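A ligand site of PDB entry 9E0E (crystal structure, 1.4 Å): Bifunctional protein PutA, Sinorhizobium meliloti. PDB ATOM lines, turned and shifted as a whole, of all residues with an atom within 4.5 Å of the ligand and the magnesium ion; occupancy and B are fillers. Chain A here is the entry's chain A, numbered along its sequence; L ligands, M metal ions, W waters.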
ATOM      1  N   ILE A 705      19.135 -27.815  14.142  1.00  0.00           N
ATOM      2  CA  ILE A 705      19.113 -27.112  12.880  1.00  0.00           C
ATOM      3  C   ILE A 705      17.781 -27.413  12.219  1.00  0.00           C
ATOM      4  O   ILE A 705      17.403 -28.577  12.080  1.00  0.00           O
ATOM      5  CB  ILE A 705      20.291 -27.546  11.986  1.00  0.00           C
ATOM      6  CG1 ILE A 705      21.608 -27.121  12.639  1.00  0.00           C
ATOM      7  CG2 ILE A 705      20.169 -26.958  10.625  1.00  0.00           C
ATOM      8  CD1 ILE A 705      22.820 -27.757  11.998  1.00  0.00           C
ATOM      9  N   SER A 706      17.065 -26.367  11.838  1.00  0.00           N
ATOM     10  CA  SER A 706      15.667 -26.515  11.468  1.00  0.00           C
ATOM     11  C   SER A 706      15.412 -25.884  10.115  1.00  0.00           C
ATOM     12  O   SER A 706      16.161 -25.011   9.669  1.00  0.00           O
ATOM     13  CB  SER A 706      14.771 -25.879  12.540  1.00  0.00           C
ATOM     14  OG  SER A 706      15.131 -24.536  12.753  1.00  0.00           O
ATOM     15  N   PRO A 707      14.357 -26.311   9.435  1.00  0.00           N
ATOM     16  CA  PRO A 707      14.064 -25.814   8.079  1.00  0.00           C
ATOM     17  C   PRO A 707      13.180 -24.579   8.161  1.00  0.00           C
ATOM     18  O   PRO A 707      12.588 -24.256   9.189  1.00  0.00           O
ATOM     19  CB  PRO A 707      13.273 -26.996   7.495  1.00  0.00           C
ATOM     20  CG  PRO A 707      12.512 -27.506   8.659  1.00  0.00           C
ATOM     21  CD  PRO A 707      13.433 -27.375   9.844  1.00  0.00           C
ATOM     22  N   TRP A 708      13.092 -23.875   7.036  1.00  0.00           N
ATOM     23  CA  TRP A 708      12.289 -22.656   7.030  1.00  0.00           C
ATOM     24  C   TRP A 708      10.793 -22.950   6.992  1.00  0.00           C
ATOM     25  O   TRP A 708      10.001 -22.132   7.436  1.00  0.00           O
ATOM     26  CB  TRP A 708      12.664 -21.755   5.853  1.00  0.00           C
ATOM     27  CG  TRP A 708      12.117 -22.282   4.573  1.00  0.00           C
ATOM     28  CD1 TRP A 708      12.762 -23.094   3.680  1.00  0.00           C
ATOM     29  CD2 TRP A 708      10.791 -22.099   4.065  1.00  0.00           C
ATOM     30  NE1 TRP A 708      11.915 -23.407   2.644  1.00  0.00           N
ATOM     31  CE2 TRP A 708      10.704 -22.822   2.864  1.00  0.00           C
ATOM     32  CE3 TRP A 708       9.673 -21.382   4.511  1.00  0.00           C
ATOM     33  CZ2 TRP A 708       9.540 -22.861   2.095  1.00  0.00           C
ATOM     34  CZ3 TRP A 708       8.514 -21.431   3.757  1.00  0.00           C
ATOM     35  CH2 TRP A 708       8.461 -22.155   2.558  1.00  0.00           C
ATOM     36  N   ASN A 709      10.397 -24.118   6.475  1.00  0.00           N
ATOM     37  CA  ASN A 709       9.028 -24.267   5.993  1.00  0.00           C
ATOM     38  C   ASN A 709       8.048 -24.549   7.115  1.00  0.00           C
ATOM     39  O   ASN A 709       6.854 -24.296   6.953  1.00  0.00           O
ATOM     40  CB  ASN A 709       8.965 -25.364   4.947  1.00  0.00           C
ATOM     41  CG  ASN A 709       9.183 -26.719   5.534  1.00  0.00           C
ATOM     42  OD1 ASN A 709      10.245 -27.011   6.069  1.00  0.00           O
ATOM     43  ND2 ASN A 709       8.165 -27.558   5.462  1.00  0.00           N
ATOM     44  N   PHE A 710       8.517 -25.102   8.216  1.00  0.00           N
ATOM     45  CA  PHE A 710       7.747 -25.231   9.446  1.00  0.00           C
ATOM     46  C   PHE A 710       8.544 -24.467  10.494  1.00  0.00           C
ATOM     47  O   PHE A 710       9.163 -25.058  11.388  1.00  0.00           O
ATOM     48  CB  PHE A 710       7.568 -26.694   9.853  1.00  0.00           C
ATOM     49  CG  PHE A 710       6.773 -27.507   8.866  1.00  0.00           C
ATOM     50  CD1 PHE A 710       5.708 -26.947   8.171  1.00  0.00           C
ATOM     51  CD2 PHE A 710       7.109 -28.834   8.625  1.00  0.00           C
ATOM     52  CE1 PHE A 710       4.978 -27.716   7.261  1.00  0.00           C
ATOM     53  CE2 PHE A 710       6.372 -29.596   7.730  1.00  0.00           C
ATOM     54  CZ  PHE A 710       5.312 -29.033   7.056  1.00  0.00           C
ATOM     55  N   ILE A 714       8.660 -27.332  13.783  1.00  0.00           N
ATOM     56  CA  ILE A 714       9.828 -28.207  13.819  1.00  0.00           C
ATOM     57  C   ILE A 714      10.928 -27.595  14.669  1.00  0.00           C
ATOM     58  O   ILE A 714      11.599 -28.292  15.432  1.00  0.00           O
ATOM     59  CB  ILE A 714      10.305 -28.540  12.393  1.00  0.00           C
ATOM     60  CG1 ILE A 714       9.196 -29.354  11.706  1.00  0.00           C
ATOM     61  CG2 ILE A 714      11.654 -29.278  12.434  1.00  0.00           C
ATOM     62  CD1 ILE A 714       9.664 -30.506  10.859  1.00  0.00           C
ATOM     63  N   LYS A 732      19.687 -23.259  15.750  1.00  0.00           N
ATOM     64  CA  LYS A 732      20.067 -22.584  14.516  1.00  0.00           C
ATOM     65  C   LYS A 732      18.873 -22.640  13.568  1.00  0.00           C
ATOM     66  O   LYS A 732      18.700 -23.626  12.849  1.00  0.00           O
ATOM     67  CB  LYS A 732      21.295 -23.245  13.888  1.00  0.00           C
ATOM     68  CG  LYS A 732      22.235 -22.296  13.168  1.00  0.00           C
ATOM     69  CD  LYS A 732      21.547 -21.566  12.023  1.00  0.00           C
ATOM     70  CE  LYS A 732      21.273 -22.526  10.866  1.00  0.00           C
ATOM     71  NZ  LYS A 732      20.553 -21.795   9.783  1.00  0.00           N
ATOM     72  N   PRO A 733      18.031 -21.615  13.547  1.00  0.00           N
ATOM     73  CA  PRO A 733      16.881 -21.617  12.647  1.00  0.00           C
ATOM     74  C   PRO A 733      17.318 -21.312  11.230  1.00  0.00           C
ATOM     75  O   PRO A 733      18.379 -20.727  10.983  1.00  0.00           O
ATOM     76  CB  PRO A 733      16.033 -20.453  13.180  1.00  0.00           C
ATOM     77  CG  PRO A 733      17.037 -19.500  13.720  1.00  0.00           C
ATOM     78  CD  PRO A 733      18.137 -20.360  14.307  1.00  0.00           C
ATOM     79  N   ALA A 734      16.486 -21.738  10.287  1.00  0.00           N
ATOM     80  CA  ALA A 734      16.742 -21.447   8.887  1.00  0.00           C
ATOM     81  C   ALA A 734      16.922 -19.951   8.673  1.00  0.00           C
ATOM     82  O   ALA A 734      16.274 -19.125   9.340  1.00  0.00           O
ATOM     83  CB  ALA A 734      15.575 -21.947   8.032  1.00  0.00           C
ATOM     84  N   GLU A 735      17.805 -19.606   7.748  1.00  0.00           N
ATOM     85  CA  GLU A 735      18.078 -18.202   7.484  1.00  0.00           C
ATOM     86  C   GLU A 735      16.843 -17.460   6.981  1.00  0.00           C
ATOM     87  O   GLU A 735      16.764 -16.234   7.154  1.00  0.00           O
ATOM     88  CB  GLU A 735      19.238 -18.054   6.506  1.00  0.00           C
ATOM     89  CG  GLU A 735      19.071 -18.780   5.179  1.00  0.00           C
ATOM     90  CD  GLU A 735      19.598 -20.214   5.205  1.00  0.00           C
ATOM     91  OE1 GLU A 735      19.603 -20.828   6.295  1.00  0.00           O
ATOM     92  OE2 GLU A 735      20.005 -20.724   4.133  1.00  0.00           O
ATOM     93  N   GLU A 736      15.888 -18.159   6.382  1.00  0.00           N
ATOM     94  CA  GLU A 736      14.706 -17.490   5.850  1.00  0.00           C
ATOM     95  C   GLU A 736      13.747 -17.043   6.949  1.00  0.00           C
ATOM     96  O   GLU A 736      13.002 -16.070   6.753  1.00  0.00           O
ATOM     97  CB  GLU A 736      13.967 -18.385   4.861  1.00  0.00           C
ATOM     98  CG  GLU A 736      14.778 -18.760   3.637  1.00  0.00           C
ATOM     99  CD  GLU A 736      15.565 -20.043   3.816  1.00  0.00           C
ATOM    100  OE1 GLU A 736      15.754 -20.485   4.970  1.00  0.00           O
ATOM    101  OE2 GLU A 736      15.979 -20.634   2.788  1.00  0.00           O
ATOM    102  N   GLY A 763      21.300 -17.336  11.389  1.00  0.00           N
ATOM    103  CA  GLY A 763      22.283 -17.307  10.329  1.00  0.00           C
ATOM    104  C   GLY A 763      22.019 -18.422   9.340  1.00  0.00           C
ATOM    105  O   GLY A 763      21.045 -19.162   9.441  1.00  0.00           O
ATOM    106  N   ASP A 764      22.920 -18.523   8.359  1.00  0.00           N
ATOM    107  CA  ASP A 764      22.741 -19.457   7.267  1.00  0.00           C
ATOM    108  C   ASP A 764      23.420 -20.793   7.585  1.00  0.00           C
ATOM    109  O   ASP A 764      23.687 -21.109   8.745  1.00  0.00           O
ATOM    110  CB  ASP A 764      23.184 -18.810   5.951  1.00  0.00           C
ATOM    111  CG  ASP A 764      24.649 -18.391   5.966  1.00  0.00           C
ATOM    112  OD1 ASP A 764      25.416 -18.891   6.818  1.00  0.00           O
ATOM    113  OD2 ASP A 764      25.032 -17.541   5.135  1.00  0.00           O
ATOM    114  N   GLY A 765      23.710 -21.577   6.552  1.00  0.00           N
ATOM    115  CA  GLY A 765      24.298 -22.900   6.745  1.00  0.00           C
ATOM    116  C   GLY A 765      25.680 -22.853   7.356  1.00  0.00           C
ATOM    117  O   GLY A 765      26.093 -23.833   7.986  1.00  0.00           O
ATOM    118  N   GLY A 768      25.113 -23.152  10.980  1.00  0.00           N
ATOM    119  CA  GLY A 768      24.834 -24.547  11.244  1.00  0.00           C
ATOM    120  C   GLY A 768      26.088 -25.398  11.194  1.00  0.00           C
ATOM    121  O   GLY A 768      26.332 -26.208  12.088  1.00  0.00           O
ATOM    122  N   ALA A 769      26.887 -25.216  10.154  1.00  0.00           N
ATOM    123  CA  ALA A 769      28.085 -26.042   9.989  1.00  0.00           C
ATOM    124  C   ALA A 769      29.088 -25.768  11.104  1.00  0.00           C
ATOM    125  O   ALA A 769      29.730 -26.698  11.601  1.00  0.00           O
ATOM    126  CB  ALA A 769      28.715 -25.799   8.609  1.00  0.00           C
ATOM    127  N   PHE A 782      18.688 -32.479  12.968  1.00  0.00           N
ATOM    128  CA  PHE A 782      18.591 -31.790  11.700  1.00  0.00           C
ATOM    129  C   PHE A 782      17.276 -32.153  11.029  1.00  0.00           C
ATOM    130  O   PHE A 782      16.957 -33.337  10.871  1.00  0.00           O
ATOM    131  CB  PHE A 782      19.698 -32.212  10.746  1.00  0.00           C
ATOM    132  CG  PHE A 782      19.576 -31.599   9.386  1.00  0.00           C
ATOM    133  CD1 PHE A 782      19.966 -30.286   9.174  1.00  0.00           C
ATOM    134  CD2 PHE A 782      19.024 -32.316   8.328  1.00  0.00           C
ATOM    135  CE1 PHE A 782      19.847 -29.710   7.947  1.00  0.00           C
ATOM    136  CE2 PHE A 782      18.893 -31.736   7.093  1.00  0.00           C
ATOM    137  CZ  PHE A 782      19.306 -30.432   6.896  1.00  0.00           C
ATOM    138  N   THR A 783      16.557 -31.132  10.596  1.00  0.00           N
ATOM    139  CA  THR A 783      15.446 -31.314   9.673  1.00  0.00           C
ATOM    140  C   THR A 783      15.670 -30.348   8.534  1.00  0.00           C
ATOM    141  O   THR A 783      15.923 -29.163   8.752  1.00  0.00           O
ATOM    142  CB  THR A 783      14.108 -31.044  10.376  1.00  0.00           C
ATOM    143  OG1 THR A 783      13.974 -31.936  11.483  1.00  0.00           O
ATOM    144  CG2 THR A 783      12.973 -31.302   9.426  1.00  0.00           C
ATOM    145  N   GLY A 784      15.634 -30.878   7.313  1.00  0.00           N
ATOM    146  CA  GLY A 784      15.972 -30.088   6.149  1.00  0.00           C
ATOM    147  C   GLY A 784      16.141 -31.000   4.958  1.00  0.00           C
ATOM    148  O   GLY A 784      15.674 -32.132   4.972  1.00  0.00           O
ATOM    149  N   SER A 785      16.835 -30.492   3.946  1.00  0.00           N
ATOM    150  CA  SER A 785      17.008 -31.267   2.729  1.00  0.00           C
ATOM    151  C   SER A 785      17.964 -32.436   2.933  1.00  0.00           C
ATOM    152  O   SER A 785      18.869 -32.405   3.770  1.00  0.00           O
ATOM    153  CB  SER A 785      17.548 -30.365   1.619  1.00  0.00           C
ATOM    154  OG  SER A 785      18.840 -29.888   1.926  1.00  0.00           O
ATOM    155  N   VAL A 788      21.698 -31.460   2.411  1.00  0.00           N
ATOM    156  CA  VAL A 788      22.372 -30.818   3.535  1.00  0.00           C
ATOM    157  C   VAL A 788      22.629 -31.830   4.644  1.00  0.00           C
ATOM    158  O   VAL A 788      23.721 -31.848   5.241  1.00  0.00           O
ATOM    159  CB  VAL A 788      21.556 -29.606   4.024  1.00  0.00           C
ATOM    160  CG1 VAL A 788      22.124 -29.102   5.340  1.00  0.00           C
ATOM    161  CG2 VAL A 788      21.604 -28.508   2.976  1.00  0.00           C
ATOM    162  N   LEU A 791      25.788 -33.533   3.981  1.00  0.00           N
ATOM    163  CA  LEU A 791      26.949 -32.749   4.370  1.00  0.00           C
ATOM    164  C   LEU A 791      27.194 -32.833   5.870  1.00  0.00           C
ATOM    165  O   LEU A 791      28.339 -32.957   6.322  1.00  0.00           O
ATOM    166  CB  LEU A 791      26.763 -31.304   3.954  1.00  0.00           C
ATOM    167  CG  LEU A 791      26.730 -31.038   2.443  1.00  0.00           C
ATOM    168  CD1 LEU A 791      26.288 -29.627   2.158  1.00  0.00           C
ATOM    169  CD2 LEU A 791      28.092 -31.318   1.833  1.00  0.00           C
ATOM    170  N   ILE A 792      26.124 -32.782   6.668  1.00  0.00           N
ATOM    171  CA  ILE A 792      26.285 -32.898   8.111  1.00  0.00           C
ATOM    172  C   ILE A 792      26.797 -34.289   8.494  1.00  0.00           C
ATOM    173  O   ILE A 792      27.700 -34.429   9.320  1.00  0.00           O
ATOM    174  CB  ILE A 792      24.965 -32.556   8.820  1.00  0.00           C
ATOM    175  CG1 ILE A 792      24.685 -31.072   8.649  1.00  0.00           C
ATOM    176  CG2 ILE A 792      25.027 -32.922  10.305  1.00  0.00           C
ATOM    177  CD1 ILE A 792      23.272 -30.688   9.000  1.00  0.00           C
ATOM    178  N   GLU A 812      16.009 -35.650   9.531  1.00  0.00           N
ATOM    179  CA  GLU A 812      14.685 -35.840   8.971  1.00  0.00           C
ATOM    180  C   GLU A 812      14.631 -35.012   7.700  1.00  0.00           C
ATOM    181  O   GLU A 812      14.767 -33.793   7.736  1.00  0.00           O
ATOM    182  CB  GLU A 812      13.648 -35.433  10.013  1.00  0.00           C
ATOM    183  CG  GLU A 812      13.736 -36.321  11.275  1.00  0.00           C
ATOM    184  CD  GLU A 812      13.605 -37.820  10.945  1.00  0.00           C
ATOM    185  OE1 GLU A 812      12.459 -38.286  10.818  1.00  0.00           O
ATOM    186  OE2 GLU A 812      14.642 -38.514  10.807  1.00  0.00           O
ATOM    187  N   THR A 813      14.483 -35.694   6.562  1.00  0.00           N
ATOM    188  CA  THR A 813      14.819 -35.085   5.286  1.00  0.00           C
ATOM    189  C   THR A 813      13.669 -35.109   4.278  1.00  0.00           C
ATOM    190  O   THR A 813      12.510 -35.195   4.679  1.00  0.00           O
ATOM    191  CB  THR A 813      16.135 -35.675   4.746  1.00  0.00           C
ATOM    192  OG1 THR A 813      16.077 -37.109   4.780  1.00  0.00           O
ATOM    193  CG2 THR A 813      17.288 -35.235   5.639  1.00  0.00           C
ATOM    194  N   GLY A 814      13.984 -35.022   2.983  1.00  0.00           N
ATOM    195  CA  GLY A 814      12.979 -34.754   1.974  1.00  0.00           C
ATOM    196  C   GLY A 814      12.113 -35.956   1.647  1.00  0.00           C
ATOM    197  O   GLY A 814      12.325 -37.069   2.114  1.00  0.00           O
ATOM    198  N   GLY A 815      11.110 -35.702   0.800  1.00  0.00           N
ATOM    199  CA  GLY A 815      10.201 -36.737   0.374  1.00  0.00           C
ATOM    200  C   GLY A 815       9.967 -36.658  -1.118  1.00  0.00           C
ATOM    201  O   GLY A 815      10.267 -35.651  -1.767  1.00  0.00           O
ATOM    202  N   CYS A 846       7.213 -30.932   3.750  1.00  0.00           N
ATOM    203  CA  CYS A 846       7.981 -32.120   3.401  1.00  0.00           C
ATOM    204  C   CYS A 846       7.059 -33.287   3.059  1.00  0.00           C
ATOM    205  O   CYS A 846       7.435 -34.164   2.294  1.00  0.00           O
ATOM    206  CB  CYS A 846       8.895 -32.502   4.553  1.00  0.00           C
ATOM    207  SG  CYS A 846       8.053 -32.615   6.128  1.00  0.00           S
ATOM    208  N   GLU A 942      13.479 -34.380  -4.907  1.00  0.00           N
ATOM    209  CA  GLU A 942      12.337 -33.621  -4.424  1.00  0.00           C
ATOM    210  C   GLU A 942      12.330 -32.231  -5.032  1.00  0.00           C
ATOM    211  O   GLU A 942      13.364 -31.548  -5.082  1.00  0.00           O
ATOM    212  CB  GLU A 942      12.469 -33.516  -2.904  1.00  0.00           C
ATOM    213  CG  GLU A 942      11.462 -32.621  -2.213  1.00  0.00           C
ATOM    214  CD  GLU A 942      11.844 -32.379  -0.776  1.00  0.00           C
ATOM    215  OE1 GLU A 942      12.969 -31.858  -0.555  1.00  0.00           O
ATOM    216  OE2 GLU A 942      11.055 -32.708   0.128  1.00  0.00           O
ATOM    217  N   PHE A 944      10.604 -28.912  -4.137  1.00  0.00           N
ATOM    218  CA  PHE A 944       9.929 -28.406  -2.939  1.00  0.00           C
ATOM    219  C   PHE A 944       9.142 -27.167  -3.320  1.00  0.00           C
ATOM    220  O   PHE A 944       9.548 -26.023  -3.074  1.00  0.00           O
ATOM    221  CB  PHE A 944      10.952 -28.120  -1.844  1.00  0.00           C
ATOM    222  CG  PHE A 944      10.380 -28.069  -0.470  1.00  0.00           C
ATOM    223  CD1 PHE A 944       9.894 -29.213   0.138  1.00  0.00           C
ATOM    224  CD2 PHE A 944      10.337 -26.878   0.242  1.00  0.00           C
ATOM    225  CE1 PHE A 944       9.374 -29.161   1.423  1.00  0.00           C
ATOM    226  CE2 PHE A 944       9.827 -26.844   1.540  1.00  0.00           C
ATOM    227  CZ  PHE A 944       9.338 -27.978   2.120  1.00  0.00           C
ATOM    228  N   LEU A 972       8.774 -40.967   2.923  1.00  0.00           N
ATOM    229  CA  LEU A 972       8.227 -40.078   3.933  1.00  0.00           C
ATOM    230  C   LEU A 972       6.724 -40.285   4.056  1.00  0.00           C
ATOM    231  O   LEU A 972       6.295 -41.081   4.896  1.00  0.00           O
ATOM    232  CB  LEU A 972       8.597 -38.632   3.621  1.00  0.00           C
ATOM    233  CG  LEU A 972       8.266 -37.647   4.736  1.00  0.00           C
ATOM    234  CD1 LEU A 972       8.838 -38.098   6.083  1.00  0.00           C
ATOM    235  CD2 LEU A 972       8.834 -36.282   4.374  1.00  0.00           C
ATOM    236  N   PHE A1012       5.693 -38.550  13.140  1.00  0.00           N
ATOM    237  CA  PHE A1012       6.012 -38.169  11.785  1.00  0.00           C
ATOM    238  C   PHE A1012       7.476 -38.386  11.505  1.00  0.00           C
ATOM    239  O   PHE A1012       8.335 -37.961  12.272  1.00  0.00           O
ATOM    240  CB  PHE A1012       5.634 -36.713  11.500  1.00  0.00           C
ATOM    241  CG  PHE A1012       5.771 -36.370  10.068  1.00  0.00           C
ATOM    242  CD1 PHE A1012       4.760 -36.677   9.171  1.00  0.00           C
ATOM    243  CD2 PHE A1012       6.938 -35.792   9.593  1.00  0.00           C
ATOM    244  CE1 PHE A1012       4.902 -36.405   7.834  1.00  0.00           C
ATOM    245  CE2 PHE A1012       7.080 -35.495   8.257  1.00  0.00           C
ATOM    246  CZ  PHE A1012       6.068 -35.804   7.375  1.00  0.00           C
ATOM    247  N   SER A1018      14.500 -40.127   3.293  1.00  0.00           N
ATOM    248  CA  SER A1018      13.613 -39.224   4.014  1.00  0.00           C
ATOM    249  C   SER A1018      13.897 -39.135   5.499  1.00  0.00           C
ATOM    250  O   SER A1018      13.289 -38.294   6.169  1.00  0.00           O
ATOM    251  CB  SER A1018      12.158 -39.656   3.828  1.00  0.00           C
ATOM    252  OG  SER A1018      11.828 -39.645   2.460  1.00  0.00           O
HETATM  253  P1  LIG L   1      17.699 -26.814   4.012  1.00  0.00           P
HETATM  254  O1  LIG L   1      18.405 -28.168   3.770  1.00  0.00           O
HETATM  255  O2  LIG L   1      17.831 -25.792   2.977  1.00  0.00           O
HETATM  256  O3  LIG L   1      18.075 -26.064   5.232  1.00  0.00           O
HETATM  257  C1  LIG L   1      17.816 -26.632   6.486  1.00  0.00           C
HETATM  258  C2  LIG L   1      18.710 -26.070   7.598  1.00  0.00           C
HETATM  259  O4  LIG L   1      20.041 -26.514   7.451  1.00  0.00           O
HETATM  260  C3  LIG L   1      18.727 -24.571   7.694  1.00  0.00           C
HETATM  261  O5  LIG L   1      18.702 -24.169   9.017  1.00  0.00           O
HETATM  262  C4  LIG L   1      20.005 -24.228   7.026  1.00  0.00           C
HETATM  263  O6  LIG L   1      20.495 -22.994   7.446  1.00  0.00           O
HETATM  264  C5  LIG L   1      20.848 -25.358   7.474  1.00  0.00           C
HETATM  265  N1  LIG L   1      22.018 -25.619   6.676  1.00  0.00           N
HETATM  266  C6  LIG L   1      22.235 -25.404   5.326  1.00  0.00           C
HETATM  267  N2  LIG L   1      23.450 -25.826   4.989  1.00  0.00           N
HETATM  268  C7  LIG L   1      24.073 -26.346   6.122  1.00  0.00           C
HETATM  269  C8  LIG L   1      25.303 -26.929   6.372  1.00  0.00           C
HETATM  270  N3  LIG L   1      26.259 -27.076   5.320  1.00  0.00           N
HETATM  271  N4  LIG L   1      25.568 -27.345   7.618  1.00  0.00           N
HETATM  272  C9  LIG L   1      24.700 -27.222   8.646  1.00  0.00           C
HETATM  273  N5  LIG L   1      23.490 -26.663   8.445  1.00  0.00           N
HETATM  274  C10 LIG L   1      23.173 -26.235   7.204  1.00  0.00           C
HETATM  275  O7  LIG L   1      16.213 -26.973   4.153  1.00  0.00           O
HETATM  276  P2  LIG L   1      14.981 -25.959   4.072  1.00  0.00           P
HETATM  277  O8  LIG L   1      14.860 -25.417   2.680  1.00  0.00           O
HETATM  278  O9  LIG L   1      15.076 -24.925   5.152  1.00  0.00           O
HETATM  279  O10 LIG L   1      13.731 -26.893   4.378  1.00  0.00           O
HETATM  280  C11 LIG L   1      13.134 -27.665   3.363  1.00  0.00           C
HETATM  281  C12 LIG L   1      13.566 -29.128   3.417  1.00  0.00           C
HETATM  282  O11 LIG L   1      13.314 -29.668   4.680  1.00  0.00           O
HETATM  283  C13 LIG L   1      12.841 -29.940   2.406  1.00  0.00           C
HETATM  284  O12 LIG L   1      13.687 -30.777   1.737  1.00  0.00           O
HETATM  285  C14 LIG L   1      11.888 -30.694   3.230  1.00  0.00           C
HETATM  286  O13 LIG L   1      11.426 -31.869   2.645  1.00  0.00           O
HETATM  287  C15 LIG L   1      12.683 -30.905   4.479  1.00  0.00           C
HETATM  288  N6  LIG L   1      11.837 -31.170   5.603  1.00  0.00           N
HETATM  289  C16 LIG L   1      11.740 -32.471   6.140  1.00  0.00           C
HETATM  290  C17 LIG L   1      10.881 -32.681   7.196  1.00  0.00           C
HETATM  291  C18 LIG L   1      10.727 -34.035   7.796  1.00  0.00           C
HETATM  292  O14 LIG L   1      10.019 -34.142   8.790  1.00  0.00           O
HETATM  293  N7  LIG L   1      11.355 -35.156   7.202  1.00  0.00           N
HETATM  294  C19 LIG L   1      10.157 -31.601   7.746  1.00  0.00           C
HETATM  295  C20 LIG L   1      10.221 -30.310   7.186  1.00  0.00           C
HETATM  296  C21 LIG L   1      11.069 -30.118   6.106  1.00  0.00           C
HETATM  297 MG    MG M   1      18.410 -24.044   2.065  1.00  0.00          MG
HETATM  298  O   HOH W   1      16.840 -22.909   5.201  1.00  0.00           O
HETATM  299  O   HOH W   2      18.780 -22.247   1.265  1.00  0.00           O
HETATM  300  O   HOH W   3      19.079 -23.219   4.025  1.00  0.00           O
HETATM  301  O   HOH W   4      16.422 -23.497   1.909  1.00  0.00           O
HETATM  302  O   HOH W   5      29.155 -28.672   5.919  1.00  0.00           O
HETATM  303  O   HOH W   6      26.026 -26.131   2.513  1.00  0.00           O
HETATM  304  O   HOH W   7      10.024 -34.402  11.365  1.00  0.00           O
HETATM  305  O   HOH W   8      11.674 -37.965   8.243  1.00  0.00           O
HETATM  306  O   HOH W   9      20.484 -24.651   2.109  1.00  0.00           O
HETATM  307  O   HOH W  10      15.480 -33.249   0.261  1.00  0.00           O
HETATM  308  O   HOH W  11      18.145 -24.961   0.295  1.00  0.00           O
HETATM  309  O   HOH W  12      14.191 -26.386   0.079  1.00  0.00           O
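The magnesium ion is bound by water W2, water W11, an oxygen (O2) of the ligand, water W4, water W9 and water W3.
OE1 of Glu 735 sits at hydrogen-bond distance from O6 of the ligand, 2.6 Å away. A nitrogen (N7) of the ligand is in hydrogen-bond range of the backbone carbonyl oxygen of Thr 813 (2.8 Å). O of Ser 706 is in hydrogen-bond range of O5 of the ligand, 2.8 Å away. The backbone NH (N) of Ser 785 is in hydrogen-bond range of an oxygen (O1) of the ligand (2.8 Å). SG of Cys 846 lies close to O14 of the ligand (3.6 Å). The side-chain carboxylate (OE1) of Glu 942 sits at hydrogen-bond distance from an oxygen (O12) of the ligand (2.6 Å). N of Trp 708 lies within hydrogen-bond range of O9 of the ligand, 2.9 Å away. An oxygen (O1) of the ligand is in hydrogen-bond range of the side-chain hydroxyl (OG) of Ser 785 (2.6 Å). NZ of Lys 732 lies within hydrogen-bond range of O6 of the ligand (2.6 Å).
The backbone carbonyl oxygen of Gly 784 sits close to an oxygen (O11) of the ligand (3.4 Å). Ile 705 touches the ligand (CG2 to O4, 3.2 Å). Pro 707 touches the ligand. OD1 of Asn 709 touches C21 of the ligand, 3.2 Å away. CD2 of Phe 710 touches C20 of the ligand, 3.7 Å away. Ile 714 touches the ligand. Pro 733 touches the ligand (C to O5, 3.9 Å). Ala 734 touches the ligand. Asp 764 touches the ligand. Gly 765 touches the ligand (CA to C7, 3.5 Å). C of Gly 768 touches C9 of the ligand, 3.4 Å away. Ala 769 touches the ligand (N to C9, 3.3 Å). CE1 of Phe 782 touches O4 of the ligand, at 3.2 Å. Thr 783 touches the ligand (CG2 to C19, 3.3 Å). CG2 of Val 788 touches O1 of the ligand, 3.3 Å away. CD1 of Ile 792 touches C9 of the ligand (3.8 Å). C of Glu 812 touches N7 of the ligand (3.3 Å). Gly 814 touches the ligand. Phe 944 touches the ligand. Leu 972 touches the ligand. Phe 1012 touches the ligand (CE2 to O14, 3.3 Å). Ser 1018 touches the ligand (O to N7, 3.8 Å). Hydrophobic or aromatic side chains within 4 Å of the ligand: Ile 705, Pro 707, Trp 708, Phe 710, Ile 714, Ala 734, Ala 769, Phe 782, Val 788, Ile 792, Phe 944, Leu 972 and Phe 1012. The nearest printed residue that does not touch the ligand is Leu 791 (4.1 Å).
The backbone NH (N) of Val 788 lies close to the side-chain hydroxyl (OG) of Ser 785. The backbone NH (N) of Leu 972 lies within hydrogen-bond range of the side-chain hydroxyl (OG) of Ser 1018 (3.4 Å). O of Ser 1018 sits at hydrogen-bond distance from N of Thr 813 (2.9 Å). The backbone NH (N) of Glu 812 lies within hydrogen-bond range of the backbone carbonyl oxygen (O) of Phe 782, 2.8 Å away. The backbone carbonyl oxygen of Lys 732 sits at hydrogen-bond distance from the backbone NH of Ser 706. The backbone carbonyl oxygen (O) of Gly 763 is in hydrogen-bond range of the side-chain amino group (NZ) of Lys 732 (2.7 Å). The backbone carbonyl oxygen (O) of Ser 706 sits at hydrogen-bond distance from the backbone NH (N) of Ala 734 (3.3 Å). The backbone NH (N) of Gly 784 lies within hydrogen-bond range of the backbone carbonyl oxygen (O) of Glu 812 (3.1 Å).
No residue comes within 4 Å of the magnesium ion.
Water W4 lies within hydrogen-bond range of O8 of the ligand and OE2 of Glu 736. Water W3 bridges the side-chain carboxylate (OE2) of Glu 735 (2.7 Å) and an oxygen (O3) of the ligand (3.2 Å). Water W1 lies within hydrogen-bond range of OE1 of Glu 736 (2.7 Å) and O9 of the ligand (2.7 Å). Water W8 lies within hydrogen-bond range of the backbone carbonyl oxygen of Ser 1018 (2.6 Å), the side-chain carboxylate of Glu 812 (2.7 Å) and a nitrogen (N7) of the ligand (3.0 Å). Water W10 bridges the side-chain carboxylate (OE1) of Glu 942 (3.0 Å) and an oxygen (O12) of the ligand (3.4 Å).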
